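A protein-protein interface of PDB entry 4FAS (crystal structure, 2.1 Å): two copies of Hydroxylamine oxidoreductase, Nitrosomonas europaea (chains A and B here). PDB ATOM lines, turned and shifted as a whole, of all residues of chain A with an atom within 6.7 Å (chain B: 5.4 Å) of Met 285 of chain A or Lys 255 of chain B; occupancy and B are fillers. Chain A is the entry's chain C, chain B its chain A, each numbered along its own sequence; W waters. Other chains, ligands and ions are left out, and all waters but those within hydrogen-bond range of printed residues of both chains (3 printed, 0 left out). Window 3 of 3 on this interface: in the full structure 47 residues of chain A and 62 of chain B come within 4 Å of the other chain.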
ATOM      1  N   LYS A 278     -10.501  -4.389  17.270  1.00  0.00           N
ATOM      2  CA  LYS A 278     -10.910  -5.505  18.112  1.00  0.00           C
ATOM      3  C   LYS A 278     -10.784  -5.145  19.596  1.00  0.00           C
ATOM      4  O   LYS A 278     -11.720  -5.433  20.395  1.00  0.00           O
ATOM      5  CB  LYS A 278     -10.030  -6.737  17.779  1.00  0.00           C
ATOM      6  CG  LYS A 278     -10.594  -8.016  18.333  1.00  0.00           C
ATOM      7  CD  LYS A 278     -12.066  -8.215  18.046  1.00  0.00           C
ATOM      8  CE  LYS A 278     -12.366  -8.784  16.630  1.00  0.00           C
ATOM      9  NZ  LYS A 278     -13.860  -9.283  16.639  1.00  0.00           N
ATOM     10  N   GLY A 280     -11.301  -2.182  21.157  1.00  0.00           N
ATOM     11  CA  GLY A 280     -12.491  -1.318  21.413  1.00  0.00           C
ATOM     12  C   GLY A 280     -13.823  -2.085  21.347  1.00  0.00           C
ATOM     13  O   GLY A 280     -14.751  -1.898  22.186  1.00  0.00           O
ATOM     14  N   LYS A 281     -13.948  -2.960  20.360  1.00  0.00           N
ATOM     15  CA  LYS A 281     -15.196  -3.713  20.187  1.00  0.00           C
ATOM     16  C   LYS A 281     -15.326  -4.750  21.366  1.00  0.00           C
ATOM     17  O   LYS A 281     -16.414  -4.937  21.898  1.00  0.00           O
ATOM     18  CB  LYS A 281     -15.216  -4.418  18.812  1.00  0.00           C
ATOM     19  CG  LYS A 281     -15.516  -3.505  17.583  1.00  0.00           C
ATOM     20  CD  LYS A 281     -16.972  -3.118  17.557  1.00  0.00           C
ATOM     21  CE  LYS A 281     -17.296  -1.794  16.709  1.00  0.00           C
ATOM     22  NZ  LYS A 281     -17.080  -0.513  17.552  1.00  0.00           N
ATOM     23  N   LEU A 282     -14.235  -5.390  21.785  1.00  0.00           N
ATOM     24  CA  LEU A 282     -14.301  -6.217  22.974  1.00  0.00           C
ATOM     25  C   LEU A 282     -14.659  -5.398  24.209  1.00  0.00           C
ATOM     26  O   LEU A 282     -15.478  -5.860  25.036  1.00  0.00           O
ATOM     27  CB  LEU A 282     -12.996  -6.984  23.213  1.00  0.00           C
ATOM     28  CG  LEU A 282     -12.711  -8.187  22.315  1.00  0.00           C
ATOM     29  CD1 LEU A 282     -11.283  -8.623  22.648  1.00  0.00           C
ATOM     30  CD2 LEU A 282     -13.686  -9.324  22.642  1.00  0.00           C
ATOM     31  N   ALA A 283     -14.082  -4.194  24.361  1.00  0.00           N
ATOM     32  CA  ALA A 283     -14.533  -3.284  25.459  1.00  0.00           C
ATOM     33  C   ALA A 283     -16.009  -2.947  25.377  1.00  0.00           C
ATOM     34  O   ALA A 283     -16.682  -2.872  26.433  1.00  0.00           O
ATOM     35  CB  ALA A 283     -13.675  -1.990  25.577  1.00  0.00           C
ATOM     36  N   GLU A 284     -16.554  -2.726  24.175  1.00  0.00           N
ATOM     37  CA  GLU A 284     -17.989  -2.522  24.048  1.00  0.00           C
ATOM     38  C   GLU A 284     -18.752  -3.770  24.455  1.00  0.00           C
ATOM     39  O   GLU A 284     -19.695  -3.695  25.245  1.00  0.00           O
ATOM     40  CB  GLU A 284     -18.370  -2.157  22.629  1.00  0.00           C
ATOM     41  CG  GLU A 284     -18.152  -0.686  22.467  1.00  0.00           C
ATOM     42  CD  GLU A 284     -17.979  -0.194  21.028  1.00  0.00           C
ATOM     43  OE1 GLU A 284     -18.513  -0.779  20.012  1.00  0.00           O
ATOM     44  OE2 GLU A 284     -17.272   0.857  20.955  1.00  0.00           O
ATOM     45  N   MET A 285     -18.312  -4.930  23.958  1.00  0.00           N
ATOM     46  CA  MET A 285     -19.026  -6.174  24.241  1.00  0.00           C
ATOM     47  C   MET A 285     -18.990  -6.616  25.698  1.00  0.00           C
ATOM     48  O   MET A 285     -19.865  -7.321  26.113  1.00  0.00           O
ATOM     49  CB  MET A 285     -18.479  -7.271  23.354  1.00  0.00           C
ATOM     50  CG  MET A 285     -18.978  -7.139  21.863  1.00  0.00           C
ATOM     51  SD  MET A 285     -18.378  -8.544  20.885  1.00  0.00           S
ATOM     52  CE  MET A 285     -16.698  -8.083  20.286  1.00  0.00           C
ATOM     53  N   ASN A 286     -17.929  -6.283  26.425  1.00  0.00           N
ATOM     54  CA  ASN A 286     -17.706  -6.708  27.775  1.00  0.00           C
ATOM     55  C   ASN A 286     -17.781  -5.647  28.840  1.00  0.00           C
ATOM     56  O   ASN A 286     -17.493  -5.952  29.992  1.00  0.00           O
ATOM     57  CB  ASN A 286     -16.335  -7.342  27.884  1.00  0.00           C
ATOM     58  CG  ASN A 286     -16.284  -8.611  27.153  1.00  0.00           C
ATOM     59  OD1 ASN A 286     -17.055  -9.496  27.449  1.00  0.00           O
ATOM     60  ND2 ASN A 286     -15.468  -8.688  26.125  1.00  0.00           N
ATOM     61  N   ARG A 287     -18.098  -4.419  28.462  1.00  0.00           N
ATOM     62  CA  ARG A 287     -18.244  -3.352  29.428  1.00  0.00           C
ATOM     63  C   ARG A 287     -19.040  -3.767  30.674  1.00  0.00           C
ATOM     64  O   ARG A 287     -18.709  -3.341  31.781  1.00  0.00           O
ATOM     65  CB  ARG A 287     -18.879  -2.116  28.802  1.00  0.00           C
ATOM     66  CG  ARG A 287     -20.122  -2.376  28.036  1.00  0.00           C
ATOM     67  CD  ARG A 287     -20.947  -1.102  27.817  1.00  0.00           C
ATOM     68  NE  ARG A 287     -20.219  -0.001  27.184  1.00  0.00           N
ATOM     69  CZ  ARG A 287     -20.315   0.330  25.891  1.00  0.00           C
ATOM     70  NH1 ARG A 287     -19.601   1.335  25.457  1.00  0.00           N
ATOM     71  NH2 ARG A 287     -21.087  -0.348  25.033  1.00  0.00           N
ATOM     72  N   ASP A 288     -20.073  -4.606  30.501  1.00  0.00           N
ATOM     73  CA  ASP A 288     -20.970  -4.936  31.608  1.00  0.00           C
ATOM     74  C   ASP A 288     -20.441  -6.101  32.449  1.00  0.00           C
ATOM     75  O   ASP A 288     -21.055  -6.543  33.409  1.00  0.00           O
ATOM     76  CB  ASP A 288     -22.415  -5.173  31.068  1.00  0.00           C
ATOM     77  CG  ASP A 288     -23.121  -3.836  30.564  1.00  0.00           C
ATOM     78  OD1 ASP A 288     -23.148  -2.806  31.335  1.00  0.00           O
ATOM     79  OD2 ASP A 288     -23.697  -3.819  29.402  1.00  0.00           O
ATOM     80  N   LYS A 289     -19.261  -6.587  32.120  1.00  0.00           N
ATOM     81  CA  LYS A 289     -18.735  -7.722  32.761  1.00  0.00           C
ATOM     82  C   LYS A 289     -17.599  -7.270  33.594  1.00  0.00           C
ATOM     83  O   LYS A 289     -17.190  -7.997  34.473  1.00  0.00           O
ATOM     84  CB  LYS A 289     -18.196  -8.737  31.746  1.00  0.00           C
ATOM     85  CG  LYS A 289     -19.222  -9.369  30.786  1.00  0.00           C
ATOM     86  CD  LYS A 289     -18.608 -10.674  30.200  1.00  0.00           C
ATOM     87  CE  LYS A 289     -19.350 -11.152  28.943  1.00  0.00           C
ATOM     88  NZ  LYS A 289     -20.611 -11.873  29.310  1.00  0.00           N
ATOM     89  N   CYS B 242     -14.025 -13.762  15.324  1.00  0.00           N
ATOM     90  CA  CYS B 242     -15.355 -13.472  15.818  1.00  0.00           C
ATOM     91  C   CYS B 242     -15.432 -13.740  17.301  1.00  0.00           C
ATOM     92  O   CYS B 242     -15.861 -12.859  18.013  1.00  0.00           O
ATOM     93  CB  CYS B 242     -16.398 -14.287  15.069  1.00  0.00           C
ATOM     94  SG  CYS B 242     -16.443 -13.822  13.381  1.00  0.00           S
ATOM     95  N   ALA B 251     -20.907 -16.519  22.903  1.00  0.00           N
ATOM     96  CA  ALA B 251     -21.698 -15.356  23.254  1.00  0.00           C
ATOM     97  C   ALA B 251     -21.152 -14.102  22.590  1.00  0.00           C
ATOM     98  O   ALA B 251     -21.908 -13.285  22.132  1.00  0.00           O
ATOM     99  CB  ALA B 251     -21.686 -15.154  24.776  1.00  0.00           C
ATOM    100  N   GLU B 252     -19.830 -13.926  22.665  1.00  0.00           N
ATOM    101  CA  GLU B 252     -19.144 -12.830  22.022  1.00  0.00           C
ATOM    102  C   GLU B 252     -19.275 -12.800  20.509  1.00  0.00           C
ATOM    103  O   GLU B 252     -19.605 -11.752  19.938  1.00  0.00           O
ATOM    104  CB  GLU B 252     -17.650 -12.827  22.437  1.00  0.00           C
ATOM    105  CG  GLU B 252     -16.752 -11.788  21.673  1.00  0.00           C
ATOM    106  CD  GLU B 252     -15.265 -12.057  21.963  1.00  0.00           C
ATOM    107  OE1 GLU B 252     -14.980 -12.461  23.115  1.00  0.00           O
ATOM    108  OE2 GLU B 252     -14.375 -11.849  21.094  1.00  0.00           O
ATOM    109  N   SER B 253     -19.005 -13.923  19.835  1.00  0.00           N
ATOM    110  CA  SER B 253     -19.114 -13.997  18.361  1.00  0.00           C
ATOM    111  C   SER B 253     -20.520 -13.737  17.866  1.00  0.00           C
ATOM    112  O   SER B 253     -20.718 -13.382  16.720  1.00  0.00           O
ATOM    113  CB  SER B 253     -18.613 -15.341  17.844  1.00  0.00           C
ATOM    114  OG  SER B 253     -19.256 -16.437  18.519  1.00  0.00           O
ATOM    115  N   ARG B 254     -21.519 -13.876  18.729  1.00  0.00           N
ATOM    116  CA  ARG B 254     -22.936 -13.619  18.391  1.00  0.00           C
ATOM    117  C   ARG B 254     -23.317 -12.122  18.384  1.00  0.00           C
ATOM    118  O   ARG B 254     -24.302 -11.740  17.752  1.00  0.00           O
ATOM    119  CB  ARG B 254     -23.897 -14.370  19.381  1.00  0.00           C
ATOM    120  CG  ARG B 254     -24.001 -15.885  19.004  1.00  0.00           C
ATOM    121  CD  ARG B 254     -24.852 -16.608  19.955  1.00  0.00           C
ATOM    122  NE  ARG B 254     -24.582 -18.052  19.970  1.00  0.00           N
ATOM    123  CZ  ARG B 254     -24.152 -18.760  21.029  1.00  0.00           C
ATOM    124  NH1 ARG B 254     -23.891 -18.211  22.219  1.00  0.00           N
ATOM    125  NH2 ARG B 254     -23.976 -20.052  20.894  1.00  0.00           N
ATOM    126  N   LYS B 255     -22.529 -11.293  19.062  1.00  0.00           N
ATOM    127  CA  LYS B 255     -22.842  -9.859  19.096  1.00  0.00           C
ATOM    128  C   LYS B 255     -22.358  -9.192  17.791  1.00  0.00           C
ATOM    129  O   LYS B 255     -21.249  -9.503  17.274  1.00  0.00           O
ATOM    130  CB  LYS B 255     -22.141  -9.278  20.267  1.00  0.00           C
ATOM    131  CG  LYS B 255     -22.530 -10.003  21.575  1.00  0.00           C
ATOM    132  CD  LYS B 255     -21.951  -9.210  22.761  1.00  0.00           C
ATOM    133  CE  LYS B 255     -22.041 -10.034  24.014  1.00  0.00           C
ATOM    134  NZ  LYS B 255     -22.086  -9.174  25.198  1.00  0.00           N
ATOM    135  N   PRO B 256     -23.156  -8.251  17.266  1.00  0.00           N
ATOM    136  CA  PRO B 256     -22.777  -7.534  16.033  1.00  0.00           C
ATOM    137  C   PRO B 256     -21.403  -6.950  16.062  1.00  0.00           C
ATOM    138  O   PRO B 256     -20.748  -6.898  15.006  1.00  0.00           O
ATOM    139  CB  PRO B 256     -23.786  -6.339  15.983  1.00  0.00           C
ATOM    140  CG  PRO B 256     -25.007  -6.847  16.671  1.00  0.00           C
ATOM    141  CD  PRO B 256     -24.456  -7.816  17.781  1.00  0.00           C
ATOM    142  N   GLU B 257     -20.944  -6.454  17.224  1.00  0.00           N
ATOM    143  CA  GLU B 257     -19.540  -5.907  17.370  1.00  0.00           C
ATOM    144  C   GLU B 257     -18.486  -6.894  16.921  1.00  0.00           C
ATOM    145  O   GLU B 257     -17.437  -6.477  16.466  1.00  0.00           O
ATOM    146  CB  GLU B 257     -19.304  -5.495  18.844  1.00  0.00           C
ATOM    147  CG  GLU B 257     -20.112  -4.267  19.414  1.00  0.00           C
ATOM    148  CD  GLU B 257     -21.627  -4.557  19.695  1.00  0.00           C
ATOM    149  OE1 GLU B 257     -22.005  -5.742  19.680  1.00  0.00           O
ATOM    150  OE2 GLU B 257     -22.431  -3.614  19.988  1.00  0.00           O
ATOM    151  N   ALA B 258     -18.718  -8.226  17.017  1.00  0.00           N
ATOM    152  CA  ALA B 258     -17.703  -9.193  16.541  1.00  0.00           C
ATOM    153  C   ALA B 258     -17.315  -8.961  15.088  1.00  0.00           C
ATOM    154  O   ALA B 258     -16.152  -9.231  14.720  1.00  0.00           O
ATOM    155  CB  ALA B 258     -18.136 -10.636  16.682  1.00  0.00           C
ATOM    156  N   CYS B 259     -18.276  -8.511  14.284  1.00  0.00           N
ATOM    157  CA  CYS B 259     -18.109  -8.476  12.806  1.00  0.00           C
ATOM    158  C   CYS B 259     -17.613  -7.134  12.321  1.00  0.00           C
ATOM    159  O   CYS B 259     -17.300  -6.999  11.126  1.00  0.00           O
ATOM    160  CB  CYS B 259     -19.441  -8.765  12.051  1.00  0.00           C
ATOM    161  SG  CYS B 259     -20.496 -10.048  12.781  1.00  0.00           S
ATOM    162  N   TRP B 292     -27.221 -13.894  25.580  1.00  0.00           N
ATOM    163  CA  TRP B 292     -26.383 -14.093  24.393  1.00  0.00           C
ATOM    164  C   TRP B 292     -25.707 -15.457  24.414  1.00  0.00           C
ATOM    165  O   TRP B 292     -25.083 -15.835  23.438  1.00  0.00           O
ATOM    166  CB  TRP B 292     -25.233 -13.121  24.427  1.00  0.00           C
ATOM    167  CG  TRP B 292     -25.690 -11.719  24.192  1.00  0.00           C
ATOM    168  CD1 TRP B 292     -25.941 -10.752  25.165  1.00  0.00           C
ATOM    169  CD2 TRP B 292     -25.956 -11.096  22.912  1.00  0.00           C
ATOM    170  NE1 TRP B 292     -26.374  -9.606  24.556  1.00  0.00           N
ATOM    171  CE2 TRP B 292     -26.401  -9.780  23.191  1.00  0.00           C
ATOM    172  CE3 TRP B 292     -25.886 -11.541  21.546  1.00  0.00           C
ATOM    173  CZ2 TRP B 292     -26.749  -8.880  22.179  1.00  0.00           C
ATOM    174  CZ3 TRP B 292     -26.218 -10.633  20.513  1.00  0.00           C
ATOM    175  CH2 TRP B 292     -26.606  -9.309  20.850  1.00  0.00           C
HETATM  176  O   HOH W   1     -14.996 -10.543  18.730  1.00  0.00           O
HETATM  177  O   HOH W   2     -14.755  -6.620  16.054  1.00  0.00           O
HETATM  178  O   HOH W   3     -21.236  -1.288  20.036  1.00  0.00           O
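The side-chain amino group (NZ) of Lys 255 of chain B sits at hydrogen-bond distance from the backbone carbonyl oxygen (O) of Met 285 of chain A (3.0 Å).
The side-chain sulfur of Met 285 of chain A lies close to the backbone carbonyl oxygen of Glu 252 of chain B (3.6 Å).
The side-chain amino group of Lys 278 of chain A is in hydrogen-bond range of the backbone carbonyl oxygen of Ala 258 of chain B, at 3.0 Å.
The side-chain amino group (NZ) of Lys 281 of chain A is in salt-bridge range of the side-chain carboxylate (OE1) of Glu 284 of chain A (2.9 Å).
The side-chain amide nitrogen (ND2) of Asn 286 of chain A is in hydrogen-bond range of the backbone carbonyl oxygen (O) of Leu 282 of chain A, at 3.0 Å.
Lys 281 of chain A touches Glu 257 of chain B.
Glu 252 of chain B touches Leu 282 of chain A.
Glu 284 of chain A touches Glu 257 of chain B (OE1 to CG, 3.9 Å).
Glu 257 of chain B touches Met 285 of chain A (CB to CG, 3.5 Å).
Met 285 of chain A touches Ala 258 of chain B (CE to N, 3.8 Å).
Printed residues of chain B within 4 Å of Lys 278 of chain A: Ala 258.
Gly 280 of chain A touches none of the printed residues of chain B.
Of the printed residues of chain B, Lys 281 of chain A touches Glu 257 (3.6 Å).
Printed residues of chain B within 4 Å of Leu 282 of chain A: Glu 252.
Of chain B, only Glu 252, Lys 255, Glu 257 and Ala 258 come within 4 Å of Met 285 of chain A.
Of chain A, only Met 285 (3.0 Å) comes within 4 Å of Lys 255 of chain B.
Of the printed residues of chain A, Ala 258 of chain B touches Lys 278 (3.0 Å) and Met 285 (3.8 Å).
The nearest printed residue of chain B that does not touch Met 285 of chain A is Cys 242 of chain B (5.4 Å).
The nearest residue of chain A that does not touch Lys 255 of chain B is Lys 289 of chain A (5.0 Å).
Of the 11 printed residues of chain B, 4 touch a printed residue of chain A.
Of the 11 printed residues of chain A, 5 touch a printed residue of chain B.
Hydrophobic or aromatic side chains of chain A that line the printed part of chain B: Leu 282 and Met 285.
Among the printed residues, 8 pairs touch across the chains.
Among the printed residues, no Asp or Glu carboxylate lies within 4 Å of a Lys or Arg side-chain nitrogen of the other chain.
No position is printed for both chains.
Of the 8 pairs that touch across the chains among the printed residues, none has its exchanged pair printed and touching as well.
Water W1 lies within hydrogen-bond range of the backbone carbonyl oxygen (O) of Cys 242 of chain B (2.6 Å), the side-chain amino group (NZ) of Lys 278 of chain A (2.7 Å) and the side-chain carboxylate (OE2) of Glu 252 of chain B (2.8 Å).
Water W3 bridges the side-chain carboxylate (OE2) of Glu 257 of chain B (2.6 Å) and the side-chain carboxylate (OE1) of Glu 284 of chain A (2.8 Å).
Water W2 lies within hydrogen-bond range of the backbone carbonyl oxygen of Glu 257 of chain B (2.7 Å), the side-chain amino group of Lys 278 of chain A (2.9 Å) and the backbone carbonyl oxygen of Ala 258 of chain B (3.2 Å).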
